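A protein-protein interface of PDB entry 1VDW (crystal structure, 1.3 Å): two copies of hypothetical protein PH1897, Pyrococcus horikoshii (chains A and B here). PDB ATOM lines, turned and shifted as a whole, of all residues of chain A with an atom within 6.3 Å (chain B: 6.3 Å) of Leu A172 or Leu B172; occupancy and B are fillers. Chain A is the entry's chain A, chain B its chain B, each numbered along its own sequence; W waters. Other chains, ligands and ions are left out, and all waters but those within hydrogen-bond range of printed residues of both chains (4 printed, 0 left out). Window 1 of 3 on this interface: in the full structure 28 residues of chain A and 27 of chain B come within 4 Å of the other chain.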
ATOM      1  N   ASN A  91     -23.917  -3.334 -15.495  1.00  0.00           N
ATOM      2  CA  ASN A  91     -23.129  -4.353 -14.822  1.00  0.00           C
ATOM      3  C   ASN A  91     -22.687  -3.879 -13.450  1.00  0.00           C
ATOM      4  O   ASN A  91     -22.839  -4.586 -12.457  1.00  0.00           O
ATOM      5  CB  ASN A  91     -21.894  -4.714 -15.649  1.00  0.00           C
ATOM      6  CG  ASN A  91     -22.232  -5.472 -16.918  1.00  0.00           C
ATOM      7  OD1 ASN A  91     -23.333  -6.014 -17.070  1.00  0.00           O
ATOM      8  ND2 ASN A  91     -21.271  -5.535 -17.828  1.00  0.00           N
ATOM      9  N   ILE A  96     -21.947  -7.031 -11.475  1.00  0.00           N
ATOM     10  CA  ILE A  96     -21.355  -7.846 -12.536  1.00  0.00           C
ATOM     11  C   ILE A  96     -19.983  -7.214 -12.797  1.00  0.00           C
ATOM     12  O   ILE A  96     -19.893  -6.054 -13.198  1.00  0.00           O
ATOM     13  CB  ILE A  96     -22.251  -7.818 -13.777  1.00  0.00           C
ATOM     14  CG1 ILE A  96     -23.641  -8.355 -13.407  1.00  0.00           C
ATOM     15  CG2 ILE A  96     -21.623  -8.634 -14.895  1.00  0.00           C
ATOM     16  CD1 ILE A  96     -24.639  -8.364 -14.543  1.00  0.00           C
ATOM     17  N   PHE A  98     -17.751  -6.463 -14.929  1.00  0.00           N
ATOM     18  CA  PHE A  98     -17.351  -6.069 -16.270  1.00  0.00           C
ATOM     19  C   PHE A  98     -17.704  -4.604 -16.473  1.00  0.00           C
ATOM     20  O   PHE A  98     -18.819  -4.277 -16.853  1.00  0.00           O
ATOM     21  CB  PHE A  98     -18.060  -6.906 -17.341  1.00  0.00           C
ATOM     22  CG  PHE A  98     -17.556  -8.312 -17.441  1.00  0.00           C
ATOM     23  CD1 PHE A  98     -16.234  -8.573 -17.790  1.00  0.00           C
ATOM     24  CD2 PHE A  98     -18.396  -9.377 -17.157  1.00  0.00           C
ATOM     25  CE1 PHE A  98     -15.760  -9.882 -17.845  1.00  0.00           C
ATOM     26  CE2 PHE A  98     -17.931 -10.686 -17.209  1.00  0.00           C
ATOM     27  CZ  PHE A  98     -16.609 -10.937 -17.552  1.00  0.00           C
ATOM     28  N   SER A 152     -16.939 -11.797 -29.168  1.00  0.00           N
ATOM     29  CA  SER A 152     -17.936 -11.014 -28.451  1.00  0.00           C
ATOM     30  C   SER A 152     -18.955 -10.746 -29.565  1.00  0.00           C
ATOM     31  O   SER A 152     -18.571 -10.423 -30.696  1.00  0.00           O
ATOM     32  CB  SER A 152     -17.333  -9.714 -27.922  1.00  0.00           C
ATOM     33  OG  SER A 152     -18.332  -8.765 -27.599  1.00  0.00           O
ATOM     34  N   TYR A 154     -22.917  -8.961 -30.416  1.00  0.00           N
ATOM     35  CA  TYR A 154     -24.112  -8.182 -30.087  1.00  0.00           C
ATOM     36  C   TYR A 154     -24.918  -7.975 -31.367  1.00  0.00           C
ATOM     37  O   TYR A 154     -24.389  -7.488 -32.369  1.00  0.00           O
ATOM     38  CB  TYR A 154     -23.759  -6.784 -29.571  1.00  0.00           C
ATOM     39  CG  TYR A 154     -23.047  -6.699 -28.241  1.00  0.00           C
ATOM     40  CD1 TYR A 154     -23.733  -6.321 -27.088  1.00  0.00           C
ATOM     41  CD2 TYR A 154     -21.677  -6.903 -28.154  1.00  0.00           C
ATOM     42  CE1 TYR A 154     -23.070  -6.137 -25.885  1.00  0.00           C
ATOM     43  CE2 TYR A 154     -21.003  -6.725 -26.952  1.00  0.00           C
ATOM     44  CZ  TYR A 154     -21.710  -6.336 -25.827  1.00  0.00           C
ATOM     45  OH  TYR A 154     -21.057  -6.119 -24.641  1.00  0.00           O
ATOM     46  N   THR A 169     -19.405 -17.559 -27.790  1.00  0.00           N
ATOM     47  CA  THR A 169     -19.626 -16.128 -27.843  1.00  0.00           C
ATOM     48  C   THR A 169     -19.685 -15.600 -26.423  1.00  0.00           C
ATOM     49  O   THR A 169     -19.959 -16.337 -25.463  1.00  0.00           O
ATOM     50  CB  THR A 169     -20.965 -15.741 -28.524  1.00  0.00           C
ATOM     51  OG1 THR A 169     -22.056 -16.268 -27.764  1.00  0.00           O
ATOM     52  CG2 THR A 169     -21.030 -16.258 -29.953  1.00  0.00           C
ATOM     53  N   ARG A 170     -19.395 -14.313 -26.310  1.00  0.00           N
ATOM     54  CA  ARG A 170     -19.477 -13.595 -25.055  1.00  0.00           C
ATOM     55  C   ARG A 170     -20.217 -12.306 -25.379  1.00  0.00           C
ATOM     56  O   ARG A 170     -20.083 -11.749 -26.476  1.00  0.00           O
ATOM     57  CB  ARG A 170     -18.090 -13.259 -24.512  1.00  0.00           C
ATOM     58  CG  ARG A 170     -17.283 -14.471 -24.062  1.00  0.00           C
ATOM     59  CD  ARG A 170     -17.836 -15.064 -22.765  1.00  0.00           C
ATOM     60  NE  ARG A 170     -17.093 -16.237 -22.307  1.00  0.00           N
ATOM     61  CZ  ARG A 170     -17.328 -17.482 -22.710  1.00  0.00           C
ATOM     62  NH1 ARG A 170     -18.286 -17.731 -23.591  1.00  0.00           N
ATOM     63  NH2 ARG A 170     -16.610 -18.483 -22.214  1.00  0.00           N
ATOM     64  N   THR A 171     -21.036 -11.862 -24.443  1.00  0.00           N
ATOM     65  CA  THR A 171     -21.759 -10.600 -24.578  1.00  0.00           C
ATOM     66  C   THR A 171     -21.642 -10.086 -23.156  1.00  0.00           C
ATOM     67  O   THR A 171     -22.454 -10.392 -22.281  1.00  0.00           O
ATOM     68  CB  THR A 171     -23.214 -10.822 -25.006  1.00  0.00           C
ATOM     69  OG1 THR A 171     -23.238 -11.596 -26.214  1.00  0.00           O
ATOM     70  CG2 THR A 171     -23.894  -9.485 -25.264  1.00  0.00           C
ATOM     71  N   LEU A 172     -20.587  -9.311 -22.931  1.00  0.00           N
ATOM     72  CA  LEU A 172     -20.263  -8.850 -21.590  1.00  0.00           C
ATOM     73  C   LEU A 172     -20.899  -7.581 -21.066  1.00  0.00           C
ATOM     74  O   LEU A 172     -20.968  -7.400 -19.852  1.00  0.00           O
ATOM     75  CB  LEU A 172     -18.737  -8.756 -21.451  1.00  0.00           C
ATOM     76  CG  LEU A 172     -17.980 -10.025 -21.858  1.00  0.00           C
ATOM     77  CD1 LEU A 172     -16.488  -9.825 -21.629  1.00  0.00           C
ATOM     78  CD2 LEU A 172     -18.491 -11.222 -21.072  1.00  0.00           C
ATOM     79  N   GLY A 173     -21.364  -6.711 -21.953  1.00  0.00           N
ATOM     80  CA  GLY A 173     -21.976  -5.479 -21.494  1.00  0.00           C
ATOM     81  C   GLY A 173     -21.007  -4.324 -21.287  1.00  0.00           C
ATOM     82  O   GLY A 173     -21.354  -3.344 -20.626  1.00  0.00           O
ATOM     83  N   ALA A 174     -19.800  -4.436 -21.839  1.00  0.00           N
ATOM     84  CA  ALA A 174     -18.789  -3.373 -21.739  1.00  0.00           C
ATOM     85  C   ALA A 174     -17.879  -3.519 -22.953  1.00  0.00           C
ATOM     86  O   ALA A 174     -16.829  -4.169 -22.896  1.00  0.00           O
ATOM     87  CB  ALA A 174     -17.989  -3.509 -20.455  1.00  0.00           C
ATOM     88  N   ILE A 175     -18.284  -2.900 -24.054  1.00  0.00           N
ATOM     89  CA  ILE A 175     -17.541  -3.007 -25.297  1.00  0.00           C
ATOM     90  C   ILE A 175     -16.068  -2.608 -25.191  1.00  0.00           C
ATOM     91  O   ILE A 175     -15.225  -3.157 -25.901  1.00  0.00           O
ATOM     92  CB  ILE A 175     -18.242  -2.193 -26.424  1.00  0.00           C
ATOM     93  CG1 ILE A 175     -17.882  -2.783 -27.787  1.00  0.00           C
ATOM     94  CG2 ILE A 175     -17.839  -0.725 -26.367  1.00  0.00           C
ATOM     95  CD1 ILE A 175     -18.485  -4.153 -28.032  1.00  0.00           C
ATOM     96  N   LEU A 177     -14.043  -3.217 -22.769  1.00  0.00           N
ATOM     97  CA  LEU A 177     -13.321  -4.387 -22.294  1.00  0.00           C
ATOM     98  C   LEU A 177     -13.254  -5.460 -23.358  1.00  0.00           C
ATOM     99  O   LEU A 177     -12.239  -6.139 -23.494  1.00  0.00           O
ATOM    100  CB  LEU A 177     -13.973  -4.974 -21.042  1.00  0.00           C
ATOM    101  CG  LEU A 177     -13.862  -4.128 -19.778  1.00  0.00           C
ATOM    102  CD1 LEU A 177     -14.459  -4.902 -18.622  1.00  0.00           C
ATOM    103  CD2 LEU A 177     -12.400  -3.785 -19.493  1.00  0.00           C
ATOM    104  N   GLU A 178     -14.327  -5.627 -24.118  1.00  0.00           N
ATOM    105  CA  GLU A 178     -14.302  -6.658 -25.134  1.00  0.00           C
ATOM    106  C   GLU A 178     -13.250  -6.336 -26.189  1.00  0.00           C
ATOM    107  O   GLU A 178     -12.537  -7.222 -26.648  1.00  0.00           O
ATOM    108  CB  GLU A 178     -15.719  -6.857 -25.681  1.00  0.00           C
ATOM    109  CG  GLU A 178     -16.541  -7.636 -24.644  1.00  0.00           C
ATOM    110  CD  GLU A 178     -18.040  -7.477 -24.768  1.00  0.00           C
ATOM    111  OE1 GLU A 178     -18.531  -6.337 -24.653  1.00  0.00           O
ATOM    112  OE2 GLU A 178     -18.731  -8.503 -24.962  1.00  0.00           O
ATOM    113  N   TYR A 181      -9.921  -7.015 -24.658  1.00  0.00           N
ATOM    114  CA  TYR A 181      -9.681  -8.453 -24.617  1.00  0.00           C
ATOM    115  C   TYR A 181      -9.188  -8.922 -25.978  1.00  0.00           C
ATOM    116  O   TYR A 181      -8.300  -9.770 -26.064  1.00  0.00           O
ATOM    117  CB  TYR A 181     -10.952  -9.209 -24.227  1.00  0.00           C
ATOM    118  CG  TYR A 181     -11.370  -9.057 -22.775  1.00  0.00           C
ATOM    119  CD1 TYR A 181     -10.585  -8.360 -21.851  1.00  0.00           C
ATOM    120  CD2 TYR A 181     -12.569  -9.610 -22.331  1.00  0.00           C
ATOM    121  CE1 TYR A 181     -10.995  -8.216 -20.518  1.00  0.00           C
ATOM    122  CE2 TYR A 181     -12.983  -9.471 -21.012  1.00  0.00           C
ATOM    123  CZ  TYR A 181     -12.194  -8.776 -20.114  1.00  0.00           C
ATOM    124  OH  TYR A 181     -12.638  -8.640 -18.819  1.00  0.00           O
ATOM    125  N   LEU A 187      -9.841 -12.945 -27.082  1.00  0.00           N
ATOM    126  CA  LEU A 187     -10.937 -13.141 -28.033  1.00  0.00           C
ATOM    127  C   LEU A 187     -10.356 -12.990 -29.433  1.00  0.00           C
ATOM    128  O   LEU A 187      -9.310 -12.359 -29.611  1.00  0.00           O
ATOM    129  CB  LEU A 187     -12.035 -12.087 -27.846  1.00  0.00           C
ATOM    130  CG  LEU A 187     -12.874 -12.136 -26.570  1.00  0.00           C
ATOM    131  CD1 LEU A 187     -13.774 -10.902 -26.517  1.00  0.00           C
ATOM    132  CD2 LEU A 187     -13.692 -13.418 -26.528  1.00  0.00           C
ATOM    133  N   ASN B  91     -12.791 -18.566 -19.629  1.00  0.00           N
ATOM    134  CA  ASN B  91     -12.624 -17.227 -19.083  1.00  0.00           C
ATOM    135  C   ASN B  91     -11.398 -17.169 -18.183  1.00  0.00           C
ATOM    136  O   ASN B  91     -10.553 -16.287 -18.321  1.00  0.00           O
ATOM    137  CB  ASN B  91     -13.849 -16.814 -18.268  1.00  0.00           C
ATOM    138  CG  ASN B  91     -15.054 -16.480 -19.124  1.00  0.00           C
ATOM    139  OD1 ASN B  91     -14.971 -16.349 -20.352  1.00  0.00           O
ATOM    140  ND2 ASN B  91     -16.191 -16.315 -18.463  1.00  0.00           N
ATOM    141  N   ILE B  96     -10.424 -13.500 -18.058  1.00  0.00           N
ATOM    142  CA  ILE B  96     -11.737 -12.859 -18.053  1.00  0.00           C
ATOM    143  C   ILE B  96     -12.285 -13.184 -16.667  1.00  0.00           C
ATOM    144  O   ILE B  96     -12.496 -14.350 -16.337  1.00  0.00           O
ATOM    145  CB  ILE B  96     -12.605 -13.441 -19.176  1.00  0.00           C
ATOM    146  CG1 ILE B  96     -11.950 -13.120 -20.526  1.00  0.00           C
ATOM    147  CG2 ILE B  96     -14.017 -12.864 -19.109  1.00  0.00           C
ATOM    148  CD1 ILE B  96     -12.667 -13.697 -21.713  1.00  0.00           C
ATOM    149  N   PHE B  98     -14.766 -13.947 -14.764  1.00  0.00           N
ATOM    150  CA  PHE B  98     -16.073 -14.542 -14.547  1.00  0.00           C
ATOM    151  C   PHE B  98     -15.915 -16.058 -14.540  1.00  0.00           C
ATOM    152  O   PHE B  98     -15.888 -16.705 -15.587  1.00  0.00           O
ATOM    153  CB  PHE B  98     -17.053 -14.117 -15.636  1.00  0.00           C
ATOM    154  CG  PHE B  98     -18.480 -14.327 -15.255  1.00  0.00           C
ATOM    155  CD1 PHE B  98     -19.120 -13.434 -14.402  1.00  0.00           C
ATOM    156  CD2 PHE B  98     -19.170 -15.440 -15.706  1.00  0.00           C
ATOM    157  CE1 PHE B  98     -20.440 -13.652 -14.002  1.00  0.00           C
ATOM    158  CE2 PHE B  98     -20.484 -15.669 -15.314  1.00  0.00           C
ATOM    159  CZ  PHE B  98     -21.120 -14.773 -14.462  1.00  0.00           C
ATOM    160  N   SER B 152     -29.520 -13.561 -19.158  1.00  0.00           N
ATOM    161  CA  SER B 152     -28.348 -14.251 -19.671  1.00  0.00           C
ATOM    162  C   SER B 152     -28.972 -15.094 -20.784  1.00  0.00           C
ATOM    163  O   SER B 152     -30.058 -15.681 -20.607  1.00  0.00           O
ATOM    164  CB  SER B 152     -27.706 -15.126 -18.596  1.00  0.00           C
ATOM    165  OG  SER B 152     -26.716 -14.395 -17.894  1.00  0.00           O
ATOM    166  N   TYR B 154     -28.091 -17.951 -23.937  1.00  0.00           N
ATOM    167  CA  TYR B 154     -27.234 -18.873 -24.670  1.00  0.00           C
ATOM    168  C   TYR B 154     -28.075 -19.541 -25.741  1.00  0.00           C
ATOM    169  O   TYR B 154     -29.117 -20.137 -25.453  1.00  0.00           O
ATOM    170  CB  TYR B 154     -26.658 -19.936 -23.737  1.00  0.00           C
ATOM    171  CG  TYR B 154     -25.568 -19.432 -22.827  1.00  0.00           C
ATOM    172  CD1 TYR B 154     -24.222 -19.597 -23.159  1.00  0.00           C
ATOM    173  CD2 TYR B 154     -25.883 -18.805 -21.628  1.00  0.00           C
ATOM    174  CE1 TYR B 154     -23.212 -19.149 -22.310  1.00  0.00           C
ATOM    175  CE2 TYR B 154     -24.891 -18.352 -20.775  1.00  0.00           C
ATOM    176  CZ  TYR B 154     -23.557 -18.529 -21.121  1.00  0.00           C
ATOM    177  OH  TYR B 154     -22.574 -18.091 -20.271  1.00  0.00           O
ATOM    178  N   THR B 169     -29.181  -8.383 -23.017  1.00  0.00           N
ATOM    179  CA  THR B 169     -28.774  -9.763 -22.793  1.00  0.00           C
ATOM    180  C   THR B 169     -27.295  -9.791 -22.427  1.00  0.00           C
ATOM    181  O   THR B 169     -26.530  -8.873 -22.754  1.00  0.00           O
ATOM    182  CB  THR B 169     -28.964 -10.677 -24.034  1.00  0.00           C
ATOM    183  OG1 THR B 169     -28.088 -10.262 -25.088  1.00  0.00           O
ATOM    184  CG2 THR B 169     -30.413 -10.640 -24.510  1.00  0.00           C
ATOM    185  N   ARG B 170     -26.913 -10.853 -21.728  1.00  0.00           N
ATOM    186  CA  ARG B 170     -25.535 -11.085 -21.325  1.00  0.00           C
ATOM    187  C   ARG B 170     -25.245 -12.548 -21.620  1.00  0.00           C
ATOM    188  O   ARG B 170     -26.142 -13.394 -21.570  1.00  0.00           O
ATOM    189  CB  ARG B 170     -25.346 -10.840 -19.818  1.00  0.00           C
ATOM    190  CG  ARG B 170     -25.510  -9.389 -19.365  1.00  0.00           C
ATOM    191  CD  ARG B 170     -24.321  -8.536 -19.792  1.00  0.00           C
ATOM    192  NE  ARG B 170     -24.465  -7.129 -19.416  1.00  0.00           N
ATOM    193  CZ  ARG B 170     -25.091  -6.207 -20.141  1.00  0.00           C
ATOM    194  NH1 ARG B 170     -25.649  -6.521 -21.300  1.00  0.00           N
ATOM    195  NH2 ARG B 170     -25.145  -4.953 -19.705  1.00  0.00           N
ATOM    196  N   THR B 171     -23.994 -12.838 -21.944  1.00  0.00           N
ATOM    197  CA  THR B 171     -23.536 -14.204 -22.188  1.00  0.00           C
ATOM    198  C   THR B 171     -22.149 -14.121 -21.575  1.00  0.00           C
ATOM    199  O   THR B 171     -21.175 -13.755 -22.231  1.00  0.00           O
ATOM    200  CB  THR B 171     -23.504 -14.526 -23.685  1.00  0.00           C
ATOM    201  OG1 THR B 171     -24.790 -14.232 -24.255  1.00  0.00           O
ATOM    202  CG2 THR B 171     -23.200 -16.007 -23.898  1.00  0.00           C
ATOM    203  N   LEU B 172     -22.078 -14.462 -20.292  1.00  0.00           N
ATOM    204  CA  LEU B 172     -20.845 -14.282 -19.539  1.00  0.00           C
ATOM    205  C   LEU B 172     -19.826 -15.403 -19.526  1.00  0.00           C
ATOM    206  O   LEU B 172     -18.664 -15.165 -19.198  1.00  0.00           O
ATOM    207  CB  LEU B 172     -21.209 -13.853 -18.113  1.00  0.00           C
ATOM    208  CG  LEU B 172     -22.156 -12.637 -18.077  1.00  0.00           C
ATOM    209  CD1 LEU B 172     -22.471 -12.256 -16.640  1.00  0.00           C
ATOM    210  CD2 LEU B 172     -21.530 -11.459 -18.817  1.00  0.00           C
ATOM    211  N   GLY B 173     -20.250 -16.614 -19.868  1.00  0.00           N
ATOM    212  CA  GLY B 173     -19.317 -17.724 -19.919  1.00  0.00           C
ATOM    213  C   GLY B 173     -19.218 -18.671 -18.735  1.00  0.00           C
ATOM    214  O   GLY B 173     -18.245 -19.414 -18.637  1.00  0.00           O
ATOM    215  N   ALA B 174     -20.191 -18.650 -17.832  1.00  0.00           N
ATOM    216  CA  ALA B 174     -20.182 -19.566 -16.688  1.00  0.00           C
ATOM    217  C   ALA B 174     -21.623 -19.672 -16.214  1.00  0.00           C
ATOM    218  O   ALA B 174     -22.062 -18.924 -15.340  1.00  0.00           O
ATOM    219  CB  ALA B 174     -19.287 -19.035 -15.571  1.00  0.00           C
ATOM    220  N   GLU B 178     -24.082 -17.572 -13.665  1.00  0.00           N
ATOM    221  CA  GLU B 178     -25.175 -16.740 -14.141  1.00  0.00           C
ATOM    222  C   GLU B 178     -26.476 -17.099 -13.414  1.00  0.00           C
ATOM    223  O   GLU B 178     -27.283 -16.221 -13.122  1.00  0.00           O
ATOM    224  CB  GLU B 178     -25.274 -16.841 -15.668  1.00  0.00           C
ATOM    225  CG  GLU B 178     -24.181 -15.973 -16.311  1.00  0.00           C
ATOM    226  CD  GLU B 178     -23.852 -16.326 -17.745  1.00  0.00           C
ATOM    227  OE1 GLU B 178     -24.238 -15.571 -18.661  1.00  0.00           O
ATOM    228  OE2 GLU B 178     -23.193 -17.356 -17.957  1.00  0.00           O
ATOM    229  N   TYR B 181     -26.347 -15.405 -10.254  1.00  0.00           N
ATOM    230  CA  TYR B 181     -26.647 -13.981 -10.434  1.00  0.00           C
ATOM    231  C   TYR B 181     -28.166 -13.775 -10.423  1.00  0.00           C
ATOM    232  O   TYR B 181     -28.664 -12.796  -9.854  1.00  0.00           O
ATOM    233  CB  TYR B 181     -26.039 -13.477 -11.744  1.00  0.00           C
ATOM    234  CG  TYR B 181     -24.603 -13.015 -11.609  1.00  0.00           C
ATOM    235  CD1 TYR B 181     -23.744 -13.584 -10.667  1.00  0.00           C
ATOM    236  CD2 TYR B 181     -24.105 -11.999 -12.418  1.00  0.00           C
ATOM    237  CE1 TYR B 181     -22.426 -13.147 -10.530  1.00  0.00           C
ATOM    238  CE2 TYR B 181     -22.791 -11.560 -12.291  1.00  0.00           C
ATOM    239  CZ  TYR B 181     -21.961 -12.135 -11.344  1.00  0.00           C
ATOM    240  OH  TYR B 181     -20.673 -11.665 -11.211  1.00  0.00           O
ATOM    241  N   LEU B 187     -30.139 -10.358 -12.503  1.00  0.00           N
ATOM    242  CA  LEU B 187     -30.753 -10.655 -13.800  1.00  0.00           C
ATOM    243  C   LEU B 187     -32.187 -11.097 -13.543  1.00  0.00           C
ATOM    244  O   LEU B 187     -32.520 -11.494 -12.429  1.00  0.00           O
ATOM    245  CB  LEU B 187     -30.023 -11.811 -14.499  1.00  0.00           C
ATOM    246  CG  LEU B 187     -28.551 -11.631 -14.871  1.00  0.00           C
ATOM    247  CD1 LEU B 187     -27.967 -12.977 -15.284  1.00  0.00           C
ATOM    248  CD2 LEU B 187     -28.425 -10.612 -15.989  1.00  0.00           C
HETATM  249  O   HOH W   1     -23.657 -14.144 -27.215  1.00  0.00           O
HETATM  250  O   HOH W   2     -23.307  -3.015 -18.491  1.00  0.00           O
HETATM  251  O   HOH W   3     -26.440 -12.371 -25.546  1.00  0.00           O
HETATM  252  O   HOH W   4     -15.646 -19.582 -19.690  1.00  0.00           O
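N of Ile A96 sits at hydrogen-bond distance from O of Asn A91 (2.8 Å).
The side-chain amide nitrogen (ND2) of Asn A91 sits at hydrogen-bond distance from the backbone carbonyl oxygen (O) of Phe A98.
N of Leu A172 sits at hydrogen-bond distance from OE2 of Glu A178 (2.9 Å).
The backbone carbonyl oxygen of Asn B91 is in hydrogen-bond range of the backbone NH of Ile B96 (2.8 Å).
O of Leu B172 sits at hydrogen-bond distance from ND2 of Asn B91, at 2.8 Å.
OE1 of Glu B178 is in hydrogen-bond range of N of Leu B172.
Ile A96 touches Tyr B181, and with the chains exchanged Tyr A181 touches Ile B96.
Phe A98 touches Ile B96, but with the chains exchanged Ile A96 does not touch Phe B98 (5.2 Å).
Thr A169 touches Thr B171, and with the chains exchanged Thr A171 touches Thr B169.
Leu B172 touches its own counterpart, Leu A172.
Of the 18 pairs that touch across the chains among the printed residues, 17 have their exchanged pair printed and touching as well.
The guanidinium group (NE) of Arg B170 sits at hydrogen-bond distance from the side-chain amide oxygen (OD1) of Asn A91.
The guanidinium group (NE) of Arg A170 sits at hydrogen-bond distance from the side-chain amide oxygen (OD1) of Asn B91 (2.9 Å).
The backbone carbonyl oxygen of Thr A171 sits at hydrogen-bond distance from the backbone NH of Thr B171 (2.9 Å).
Tyr B181 touches Ile A96 (CE2 to CG1, 3.5 Å).
CZ of Phe A98 touches CG2 of Ile B96 (3.6 Å).
Arg A170 touches Thr B171.
Arg A170 touches Leu B172.
Arg A170 touches Gly B173.
CG2 of Thr A171 touches O of Thr B169, 3.7 Å away.
Leu B172 touches Thr A171 (CD2 to O, 3.7 Å).
Leu A172 touches Thr B171 (CD2 to O, 3.9 Å).
Leu A172 touches Leu B172 (CD2 to CD2, 3.8 Å).
Arg B170 touches Gly A173 (CZ to CA, 3.5 Å).
Water W3 lies within hydrogen-bond range of the side-chain hydroxyl (OG1) of Thr B169, the side-chain hydroxyl (OG1) of Thr B171 and the side-chain hydroxyl (OG1) of Thr A171.
Water W1 lies within hydrogen-bond range of OG1 of Thr A169 (2.7 Å), OG1 of Thr A171 (2.8 Å) and OG1 of Thr B171 (3.2 Å).
Water W4 lies within hydrogen-bond range of the backbone carbonyl oxygen of Gly B173, the guanidinium group of Arg A170 and the backbone NH of Asn B91.
Water W2 lies within hydrogen-bond range of O of Gly A173 (2.9 Å), NH2 of Arg B170 (2.9 Å) and N of Asn A91 (3.1 Å).
Of the printed residues of chain A, Leu B172 touches Arg A170 (3.6 Å), Thr A171 (3.7 Å) and Leu A172 (3.8 Å).
Printed residues of chain A within 4 Å of Asn B91: Arg A170.
Of the printed residues of chain B, Tyr A181 touches Ile B96 (3.8 Å).
Of the printed residues of chain A, Phe B98 touches Phe A98.
Ala A174 touches none of the printed residues of chain B.
Glu B178 touches none of the printed residues of chain A.
The nearest residue of chain B that does not touch Leu A172 is Ile B96 (4.7 Å).
The nearest printed residue of chain A that does not touch Leu B172 is Phe A98 (4.02 Å).
Of the 14 printed residues of chain B, 9 touch a printed residue of chain A.
Among the printed residues, no Asp or Glu carboxylate lies within 4 Å of a Lys or Arg side-chain nitrogen of the other chain.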
